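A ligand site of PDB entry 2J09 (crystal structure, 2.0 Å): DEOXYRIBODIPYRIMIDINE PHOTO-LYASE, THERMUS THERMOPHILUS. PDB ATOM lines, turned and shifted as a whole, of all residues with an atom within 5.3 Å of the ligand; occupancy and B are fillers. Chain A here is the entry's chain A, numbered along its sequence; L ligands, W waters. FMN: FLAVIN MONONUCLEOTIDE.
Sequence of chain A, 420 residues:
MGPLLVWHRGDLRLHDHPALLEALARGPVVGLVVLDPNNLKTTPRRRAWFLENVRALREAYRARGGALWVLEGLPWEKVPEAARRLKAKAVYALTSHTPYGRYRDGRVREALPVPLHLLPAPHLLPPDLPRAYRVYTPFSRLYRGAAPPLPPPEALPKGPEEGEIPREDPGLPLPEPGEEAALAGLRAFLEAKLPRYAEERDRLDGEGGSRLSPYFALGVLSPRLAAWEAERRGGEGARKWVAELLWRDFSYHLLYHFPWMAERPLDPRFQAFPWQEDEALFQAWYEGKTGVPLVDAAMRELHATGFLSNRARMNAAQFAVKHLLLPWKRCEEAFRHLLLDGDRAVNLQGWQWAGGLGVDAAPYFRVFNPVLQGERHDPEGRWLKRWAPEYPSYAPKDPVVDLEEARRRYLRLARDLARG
Residues that only touch the ligand: Phe 50 (3.3 Å), Leu 40 (3.4 Å), Arg 9 (3.5 Å), Leu 35 (3.5 Å), Ser 96 (3.6 Å), Leu 218 (3.6 Å), Gly 10 (3.6 Å), Gly 342 (3.8 Å), Arg 46 (3.8 Å) and Tyr 100 (3.9 Å).
15 residues have an atom within 4 Å of the ligand: Arg 9, Gly 10, Val 34, Leu 35, Asp 36, Asn 39, Leu 40, Arg 46, Phe 50, Ser 96, Thr 98, Tyr 100, Arg 104, Leu 218 and Gly 342.
The nearest printed residue that does not touch the ligand is Gly 101 (4.03 Å).
The backbone carbonyl oxygen (O) of Val 34 sits at hydrogen-bond distance from a nitrogen (N3) of the ligand, at 2.7 Å.
A nitrogen (N1) of the ligand sits close to the side-chain amide nitrogen (ND2) of Asn 39, 3.4 Å away.
OG1 of Thr 98 is in hydrogen-bond range of O2P of the ligand (2.4 Å).
The backbone NH (N) of Asp 36 sits at hydrogen-bond distance from an oxygen (O4) of the ligand, 2.9 Å away.
An oxygen (O3') of the ligand lies within hydrogen-bond range of the guanidinium group (NH1) of Arg 104 (2.5 Å).
The side-chain carboxylate of Asp 36 sits at hydrogen-bond distance from the side-chain hydroxyl of Tyr 100 (2.5 Å).
The guanidinium group (NH2) of Arg 46 sits at hydrogen-bond distance from the backbone carbonyl oxygen (O) of Gly 342, 3.0 Å away.
NH1 of Arg 46 sits at hydrogen-bond distance from OG1 of Thr 42.
The backbone carbonyl oxygen (O) of Leu 40 lies within hydrogen-bond range of the guanidinium group (NH1) of Arg 47.
N of Gly 101 lies within hydrogen-bond range of OG1 of Thr 98, 2.9 Å away.
The side-chain hydroxyl (OG1) of Thr 98 is in hydrogen-bond range of the side-chain hydroxyl (OG) of Ser 96, 3.3 Å away.
Water W2 lies within hydrogen-bond range of O2 of the ligand (2.7 Å), O of His 8 (2.7 Å), N of Val 34 (2.7 Å) and NE1 of Trp 7 (2.9 Å).
Water W3 lies within hydrogen-bond range of an oxygen (O2) of the ligand and the backbone carbonyl oxygen of Val 34.
Water W1 lies within hydrogen-bond range of the side-chain carboxylate of Asp 36 (2.6 Å), the side-chain amide nitrogen of Asn 39 (2.7 Å), the guanidinium group of Arg 104 (3.0 Å) and an oxygen (O2) of the ligand (3.4 Å).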
ATOM      1  N   TRP A   7     -14.009  27.160  34.136  1.00  0.00           N
ATOM      2  CA  TRP A   7     -14.295  26.236  33.070  1.00  0.00           C
ATOM      3  C   TRP A   7     -15.677  25.586  33.271  1.00  0.00           C
ATOM      4  O   TRP A   7     -15.903  24.862  34.259  1.00  0.00           O
ATOM      5  CB  TRP A   7     -13.131  25.213  33.039  1.00  0.00           C
ATOM      6  CG  TRP A   7     -13.348  24.114  32.062  1.00  0.00           C
ATOM      7  CD1 TRP A   7     -14.147  24.137  30.915  1.00  0.00           C
ATOM      8  CD2 TRP A   7     -12.680  22.858  32.076  1.00  0.00           C
ATOM      9  NE1 TRP A   7     -14.003  22.906  30.233  1.00  0.00           N
ATOM     10  CE2 TRP A   7     -13.140  22.105  30.947  1.00  0.00           C
ATOM     11  CE3 TRP A   7     -11.822  22.228  33.010  1.00  0.00           C
ATOM     12  CZ2 TRP A   7     -12.747  20.784  30.705  1.00  0.00           C
ATOM     13  CZ3 TRP A   7     -11.391  20.911  32.741  1.00  0.00           C
ATOM     14  CH2 TRP A   7     -11.885  20.209  31.622  1.00  0.00           C
ATOM     15  N   HIS A   8     -16.649  26.039  32.455  1.00  0.00           N
ATOM     16  CA  HIS A   8     -18.028  25.546  32.442  1.00  0.00           C
ATOM     17  C   HIS A   8     -18.121  24.279  31.607  1.00  0.00           C
ATOM     18  O   HIS A   8     -17.675  24.243  30.446  1.00  0.00           O
ATOM     19  CB  HIS A   8     -18.963  26.613  31.817  1.00  0.00           C
ATOM     20  CG  HIS A   8     -19.172  27.817  32.689  1.00  0.00           C
ATOM     21  ND1 HIS A   8     -20.262  27.958  33.516  1.00  0.00           N
ATOM     22  CD2 HIS A   8     -18.496  28.999  32.764  1.00  0.00           C
ATOM     23  CE1 HIS A   8     -20.292  29.187  34.017  1.00  0.00           C
ATOM     24  NE2 HIS A   8     -19.200  29.828  33.616  1.00  0.00           N
ATOM     25  N   ARG A   9     -18.767  23.231  32.163  1.00  0.00           N
ATOM     26  CA  ARG A   9     -18.979  22.036  31.363  1.00  0.00           C
ATOM     27  C   ARG A   9     -20.507  21.869  31.321  1.00  0.00           C
ATOM     28  O   ARG A   9     -21.212  22.697  30.735  1.00  0.00           O
ATOM     29  CB  ARG A   9     -18.198  20.837  31.976  1.00  0.00           C
ATOM     30  CG  ARG A   9     -16.673  21.049  31.870  1.00  0.00           C
ATOM     31  CD  ARG A   9     -16.066  21.670  33.168  1.00  0.00           C
ATOM     32  NE  ARG A   9     -16.083  20.735  34.294  1.00  0.00           N
ATOM     33  CZ  ARG A   9     -15.141  19.853  34.560  1.00  0.00           C
ATOM     34  NH1 ARG A   9     -14.151  19.642  33.654  1.00  0.00           N
ATOM     35  NH2 ARG A   9     -15.251  19.110  35.668  1.00  0.00           N
ATOM     36  N   GLY A  10     -21.028  20.875  32.014  1.00  0.00           N
ATOM     37  CA  GLY A  10     -22.494  20.694  32.035  1.00  0.00           C
ATOM     38  C   GLY A  10     -23.125  21.589  33.084  1.00  0.00           C
ATOM     39  O   GLY A  10     -23.772  21.111  34.054  1.00  0.00           O
ATOM     40  N   VAL A  33     -15.568  27.609  27.801  1.00  0.00           N
ATOM     41  CA  VAL A  33     -16.239  26.385  27.438  1.00  0.00           C
ATOM     42  C   VAL A  33     -15.347  25.720  26.381  1.00  0.00           C
ATOM     43  O   VAL A  33     -14.802  26.386  25.495  1.00  0.00           O
ATOM     44  CB  VAL A  33     -17.657  26.611  26.834  1.00  0.00           C
ATOM     45  CG1 VAL A  33     -18.200  25.250  26.249  1.00  0.00           C
ATOM     46  CG2 VAL A  33     -18.688  27.072  27.963  1.00  0.00           C
ATOM     47  N   VAL A  34     -15.133  24.412  26.532  1.00  0.00           N
ATOM     48  CA  VAL A  34     -14.467  23.669  25.457  1.00  0.00           C
ATOM     49  C   VAL A  34     -15.505  22.777  24.770  1.00  0.00           C
ATOM     50  O   VAL A  34     -16.176  21.949  25.438  1.00  0.00           O
ATOM     51  CB  VAL A  34     -13.249  22.802  26.008  1.00  0.00           C
ATOM     52  CG1 VAL A  34     -12.576  21.967  24.859  1.00  0.00           C
ATOM     53  CG2 VAL A  34     -12.214  23.743  26.699  1.00  0.00           C
ATOM     54  N   LEU A  35     -15.635  22.928  23.447  1.00  0.00           N
ATOM     55  CA  LEU A  35     -16.557  22.088  22.620  1.00  0.00           C
ATOM     56  C   LEU A  35     -15.769  20.782  22.335  1.00  0.00           C
ATOM     57  O   LEU A  35     -14.770  20.796  21.596  1.00  0.00           O
ATOM     58  CB  LEU A  35     -16.883  22.809  21.294  1.00  0.00           C
ATOM     59  CG  LEU A  35     -17.468  24.221  21.536  1.00  0.00           C
ATOM     60  CD1 LEU A  35     -17.749  24.928  20.161  1.00  0.00           C
ATOM     61  CD2 LEU A  35     -18.736  24.186  22.422  1.00  0.00           C
ATOM     62  N   ASP A  36     -16.132  19.726  23.060  1.00  0.00           N
ATOM     63  CA  ASP A  36     -15.330  18.524  23.174  1.00  0.00           C
ATOM     64  C   ASP A  36     -15.954  17.454  22.289  1.00  0.00           C
ATOM     65  O   ASP A  36     -17.138  17.084  22.473  1.00  0.00           O
ATOM     66  CB  ASP A  36     -15.322  18.156  24.662  1.00  0.00           C
ATOM     67  CG  ASP A  36     -14.688  16.818  24.948  1.00  0.00           C
ATOM     68  OD1 ASP A  36     -14.245  16.089  24.020  1.00  0.00           O
ATOM     69  OD2 ASP A  36     -14.566  16.516  26.155  1.00  0.00           O
ATOM     70  N   ASN A  39     -18.180  14.638  23.608  1.00  0.00           N
ATOM     71  CA  ASN A  39     -19.594  14.915  23.928  1.00  0.00           C
ATOM     72  C   ASN A  39     -20.402  15.320  22.680  1.00  0.00           C
ATOM     73  O   ASN A  39     -21.621  15.189  22.678  1.00  0.00           O
ATOM     74  CB  ASN A  39     -19.676  16.045  24.948  1.00  0.00           C
ATOM     75  CG  ASN A  39     -18.827  15.776  26.171  1.00  0.00           C
ATOM     76  OD1 ASN A  39     -18.900  14.706  26.750  1.00  0.00           O
ATOM     77  ND2 ASN A  39     -18.162  16.800  26.657  1.00  0.00           N
ATOM     78  N   LEU A  40     -19.743  15.912  21.689  1.00  0.00           N
ATOM     79  CA  LEU A  40     -20.473  16.621  20.594  1.00  0.00           C
ATOM     80  C   LEU A  40     -20.635  15.768  19.363  1.00  0.00           C
ATOM     81  O   LEU A  40     -21.260  16.180  18.365  1.00  0.00           O
ATOM     82  CB  LEU A  40     -19.781  17.971  20.229  1.00  0.00           C
ATOM     83  CG  LEU A  40     -20.105  19.081  21.253  1.00  0.00           C
ATOM     84  CD1 LEU A  40     -19.340  20.408  20.990  1.00  0.00           C
ATOM     85  CD2 LEU A  40     -21.653  19.370  21.440  1.00  0.00           C
ATOM     86  N   THR A  42     -22.574  13.635  18.351  1.00  0.00           N
ATOM     87  CA  THR A  42     -23.882  13.037  18.672  1.00  0.00           C
ATOM     88  C   THR A  42     -24.882  13.627  17.671  1.00  0.00           C
ATOM     89  O   THR A  42     -24.457  14.180  16.662  1.00  0.00           O
ATOM     90  CB  THR A  42     -24.301  13.332  20.142  1.00  0.00           C
ATOM     91  OG1 THR A  42     -25.555  12.697  20.400  1.00  0.00           O
ATOM     92  CG2 THR A  42     -24.474  14.879  20.357  1.00  0.00           C
ATOM     93  N   ARG A  46     -29.043  17.447  19.544  1.00  0.00           N
ATOM     94  CA  ARG A  46     -28.360  17.539  20.841  1.00  0.00           C
ATOM     95  C   ARG A  46     -27.141  18.475  20.741  1.00  0.00           C
ATOM     96  O   ARG A  46     -26.822  19.223  21.672  1.00  0.00           O
ATOM     97  CB  ARG A  46     -27.969  16.138  21.361  1.00  0.00           C
ATOM     98  CG  ARG A  46     -29.205  15.254  21.768  1.00  0.00           C
ATOM     99  CD  ARG A  46     -28.791  13.880  22.230  1.00  0.00           C
ATOM    100  NE  ARG A  46     -28.261  13.990  23.585  1.00  0.00           N
ATOM    101  CZ  ARG A  46     -27.240  13.280  24.023  1.00  0.00           C
ATOM    102  NH1 ARG A  46     -26.660  12.438  23.184  1.00  0.00           N
ATOM    103  NH2 ARG A  46     -26.958  13.232  25.320  1.00  0.00           N
ATOM    104  N   ARG A  47     -26.409  18.395  19.638  1.00  0.00           N
ATOM    105  CA  ARG A  47     -25.278  19.295  19.452  1.00  0.00           C
ATOM    106  C   ARG A  47     -25.804  20.732  19.490  1.00  0.00           C
ATOM    107  O   ARG A  47     -25.253  21.574  20.159  1.00  0.00           O
ATOM    108  CB  ARG A  47     -24.587  19.064  18.111  1.00  0.00           C
ATOM    109  CG  ARG A  47     -23.907  17.691  17.967  1.00  0.00           C
ATOM    110  CD  ARG A  47     -23.349  17.530  16.468  1.00  0.00           C
ATOM    111  NE  ARG A  47     -22.587  18.713  16.093  1.00  0.00           N
ATOM    112  CZ  ARG A  47     -21.258  18.805  16.160  1.00  0.00           C
ATOM    113  NH1 ARG A  47     -20.499  17.739  16.481  1.00  0.00           N
ATOM    114  NH2 ARG A  47     -20.663  19.962  15.878  1.00  0.00           N
ATOM    115  N   PHE A  50     -26.832  21.947  22.915  1.00  0.00           N
ATOM    116  CA  PHE A  50     -25.642  22.376  23.717  1.00  0.00           C
ATOM    117  C   PHE A  50     -25.053  23.696  23.191  1.00  0.00           C
ATOM    118  O   PHE A  50     -24.892  24.623  23.969  1.00  0.00           O
ATOM    119  CB  PHE A  50     -24.530  21.278  23.803  1.00  0.00           C
ATOM    120  CG  PHE A  50     -23.390  21.644  24.716  1.00  0.00           C
ATOM    121  CD1 PHE A  50     -23.457  21.366  26.093  1.00  0.00           C
ATOM    122  CD2 PHE A  50     -22.226  22.224  24.202  1.00  0.00           C
ATOM    123  CE1 PHE A  50     -22.395  21.788  26.923  1.00  0.00           C
ATOM    124  CE2 PHE A  50     -21.141  22.525  25.030  1.00  0.00           C
ATOM    125  CZ  PHE A  50     -21.279  22.401  26.365  1.00  0.00           C
ATOM    126  N   SER A  96     -16.741  16.356  38.341  1.00  0.00           N
ATOM    127  CA  SER A  96     -17.535  15.384  37.571  1.00  0.00           C
ATOM    128  C   SER A  96     -17.156  13.981  38.057  1.00  0.00           C
ATOM    129  O   SER A  96     -15.949  13.626  38.118  1.00  0.00           O
ATOM    130  CB  SER A  96     -17.228  15.454  36.076  1.00  0.00           C
ATOM    131  OG  SER A  96     -17.969  14.434  35.375  1.00  0.00           O
ATOM    132  N   THR A  98     -18.357  11.106  36.604  1.00  0.00           N
ATOM    133  CA  THR A  98     -18.556  10.132  35.520  1.00  0.00           C
ATOM    134  C   THR A  98     -17.227   9.594  35.013  1.00  0.00           C
ATOM    135  O   THR A  98     -16.175  10.171  35.250  1.00  0.00           O
ATOM    136  CB  THR A  98     -19.331  10.728  34.324  1.00  0.00           C
ATOM    137  OG1 THR A  98     -18.500  11.660  33.617  1.00  0.00           O
ATOM    138  CG2 THR A  98     -20.582  11.466  34.811  1.00  0.00           C
ATOM    139  N   TYR A 100     -16.040   9.361  32.086  1.00  0.00           N
ATOM    140  CA  TYR A 100     -15.352  10.293  31.172  1.00  0.00           C
ATOM    141  C   TYR A 100     -14.893  11.606  31.882  1.00  0.00           C
ATOM    142  O   TYR A 100     -13.755  12.081  31.682  1.00  0.00           O
ATOM    143  CB  TYR A 100     -16.183  10.620  29.908  1.00  0.00           C
ATOM    144  CG  TYR A 100     -15.466  11.650  29.066  1.00  0.00           C
ATOM    145  CD1 TYR A 100     -14.301  11.307  28.405  1.00  0.00           C
ATOM    146  CD2 TYR A 100     -15.979  12.972  28.914  1.00  0.00           C
ATOM    147  CE1 TYR A 100     -13.582  12.246  27.628  1.00  0.00           C
ATOM    148  CE2 TYR A 100     -15.268  13.930  28.160  1.00  0.00           C
ATOM    149  CZ  TYR A 100     -14.023  13.563  27.588  1.00  0.00           C
ATOM    150  OH  TYR A 100     -13.270  14.445  26.843  1.00  0.00           O
ATOM    151  N   GLY A 101     -15.745  12.144  32.714  1.00  0.00           N
ATOM    152  CA  GLY A 101     -15.431  13.331  33.494  1.00  0.00           C
ATOM    153  C   GLY A 101     -14.161  13.172  34.307  1.00  0.00           C
ATOM    154  O   GLY A 101     -13.275  14.046  34.250  1.00  0.00           O
ATOM    155  N   ARG A 104     -11.154  12.737  31.703  1.00  0.00           N
ATOM    156  CA  ARG A 104     -10.818  14.036  31.091  1.00  0.00           C
ATOM    157  C   ARG A 104     -10.117  14.940  32.172  1.00  0.00           C
ATOM    158  O   ARG A 104      -9.094  15.569  31.902  1.00  0.00           O
ATOM    159  CB  ARG A 104     -12.166  14.706  30.695  1.00  0.00           C
ATOM    160  CG  ARG A 104     -12.020  16.235  30.285  1.00  0.00           C
ATOM    161  CD  ARG A 104     -13.427  16.856  30.274  1.00  0.00           C
ATOM    162  NE  ARG A 104     -13.957  16.895  31.633  1.00  0.00           N
ATOM    163  CZ  ARG A 104     -15.265  16.950  31.942  1.00  0.00           C
ATOM    164  NH1 ARG A 104     -16.205  17.070  30.962  1.00  0.00           N
ATOM    165  NH2 ARG A 104     -15.631  16.879  33.215  1.00  0.00           N
ATOM    166  N   ALA A 217     -30.468  18.910  32.090  1.00  0.00           N
ATOM    167  CA  ALA A 217     -29.476  18.009  31.486  1.00  0.00           C
ATOM    168  C   ALA A 217     -28.179  18.721  31.172  1.00  0.00           C
ATOM    169  O   ALA A 217     -27.106  18.085  31.148  1.00  0.00           O
ATOM    170  CB  ALA A 217     -30.023  17.404  30.244  1.00  0.00           C
ATOM    171  N   LEU A 218     -28.269  20.036  30.890  1.00  0.00           N
ATOM    172  CA  LEU A 218     -27.065  20.809  30.600  1.00  0.00           C
ATOM    173  C   LEU A 218     -26.612  21.741  31.748  1.00  0.00           C
ATOM    174  O   LEU A 218     -25.721  22.577  31.554  1.00  0.00           O
ATOM    175  CB  LEU A 218     -27.250  21.632  29.342  1.00  0.00           C
ATOM    176  CG  LEU A 218     -27.552  20.922  28.015  1.00  0.00           C
ATOM    177  CD1 LEU A 218     -27.575  21.966  26.885  1.00  0.00           C
ATOM    178  CD2 LEU A 218     -26.546  19.810  27.696  1.00  0.00           C
ATOM    179  N   GLY A 342     -31.360  14.270  26.902  1.00  0.00           N
ATOM    180  CA  GLY A 342     -30.737  12.927  26.945  1.00  0.00           C
ATOM    181  C   GLY A 342     -29.494  12.938  27.820  1.00  0.00           C
ATOM    182  O   GLY A 342     -28.656  13.845  27.720  1.00  0.00           O
HETATM  183  N1  FMN L   1     -19.449  19.549  28.267  1.00  0.00           N
HETATM  184  C2  FMN L   1     -18.317  20.136  27.750  1.00  0.00           C
HETATM  185  O2  FMN L   1     -17.469  20.592  28.541  1.00  0.00           O
HETATM  186  N3  FMN L   1     -18.187  20.384  26.392  1.00  0.00           N
HETATM  187  C4  FMN L   1     -19.086  19.916  25.500  1.00  0.00           C
HETATM  188  O4  FMN L   1     -18.789  19.942  24.270  1.00  0.00           O
HETATM  189  C4A FMN L   1     -20.237  19.298  26.027  1.00  0.00           C
HETATM  190  N5  FMN L   1     -21.247  18.876  25.188  1.00  0.00           N
HETATM  191  C5A FMN L   1     -22.365  18.255  25.685  1.00  0.00           C
HETATM  192  C6  FMN L   1     -23.393  17.889  24.800  1.00  0.00           C
HETATM  193  C7  FMN L   1     -24.520  17.190  25.290  1.00  0.00           C
HETATM  194  C7M FMN L   1     -25.550  16.783  24.256  1.00  0.00           C
HETATM  195  C8  FMN L   1     -24.625  16.935  26.663  1.00  0.00           C
HETATM  196  C8M FMN L   1     -25.825  16.293  27.299  1.00  0.00           C
HETATM  197  C9  FMN L   1     -23.645  17.388  27.545  1.00  0.00           C
HETATM  198  C9A FMN L   1     -22.491  18.016  27.047  1.00  0.00           C
HETATM  199  N10 FMN L   1     -21.508  18.467  27.905  1.00  0.00           N
HETATM  200  C10 FMN L   1     -20.366  19.046  27.393  1.00  0.00           C
HETATM  201  C1' FMN L   1     -21.672  18.380  29.379  1.00  0.00           C
HETATM  202  C2' FMN L   1     -20.782  17.188  29.634  1.00  0.00           C
HETATM  203  O2' FMN L   1     -21.411  15.970  29.290  1.00  0.00           O
HETATM  204  C3' FMN L   1     -19.863  17.344  30.836  1.00  0.00           C
HETATM  205  O3' FMN L   1     -18.612  17.458  30.226  1.00  0.00           O
HETATM  206  C4' FMN L   1     -19.792  16.316  31.955  1.00  0.00           C
HETATM  207  O4' FMN L   1     -19.179  16.937  33.115  1.00  0.00           O
HETATM  208  C5' FMN L   1     -18.938  15.110  31.564  1.00  0.00           C
HETATM  209  O5' FMN L   1     -19.283  14.530  30.326  1.00  0.00           O
HETATM  210  P   FMN L   1     -20.084  13.122  30.355  1.00  0.00           P
HETATM  211  O1P FMN L   1     -19.913  12.331  29.081  1.00  0.00           O
HETATM  212  O2P FMN L   1     -19.598  12.288  31.525  1.00  0.00           O
HETATM  213  O3P FMN L   1     -21.563  13.428  30.529  1.00  0.00           O
HETATM  214  O   HOH W   1     -15.963  17.620  28.015  1.00  0.00           O
HETATM  215  O   HOH W   2     -16.331  22.987  28.501  1.00  0.00           O
HETATM  216  O   HOH W   3     -14.731  20.160  28.027  1.00  0.00           O
HETATM  217  O   HOH W   4     -24.473  17.878  31.360  1.00  0.00           O
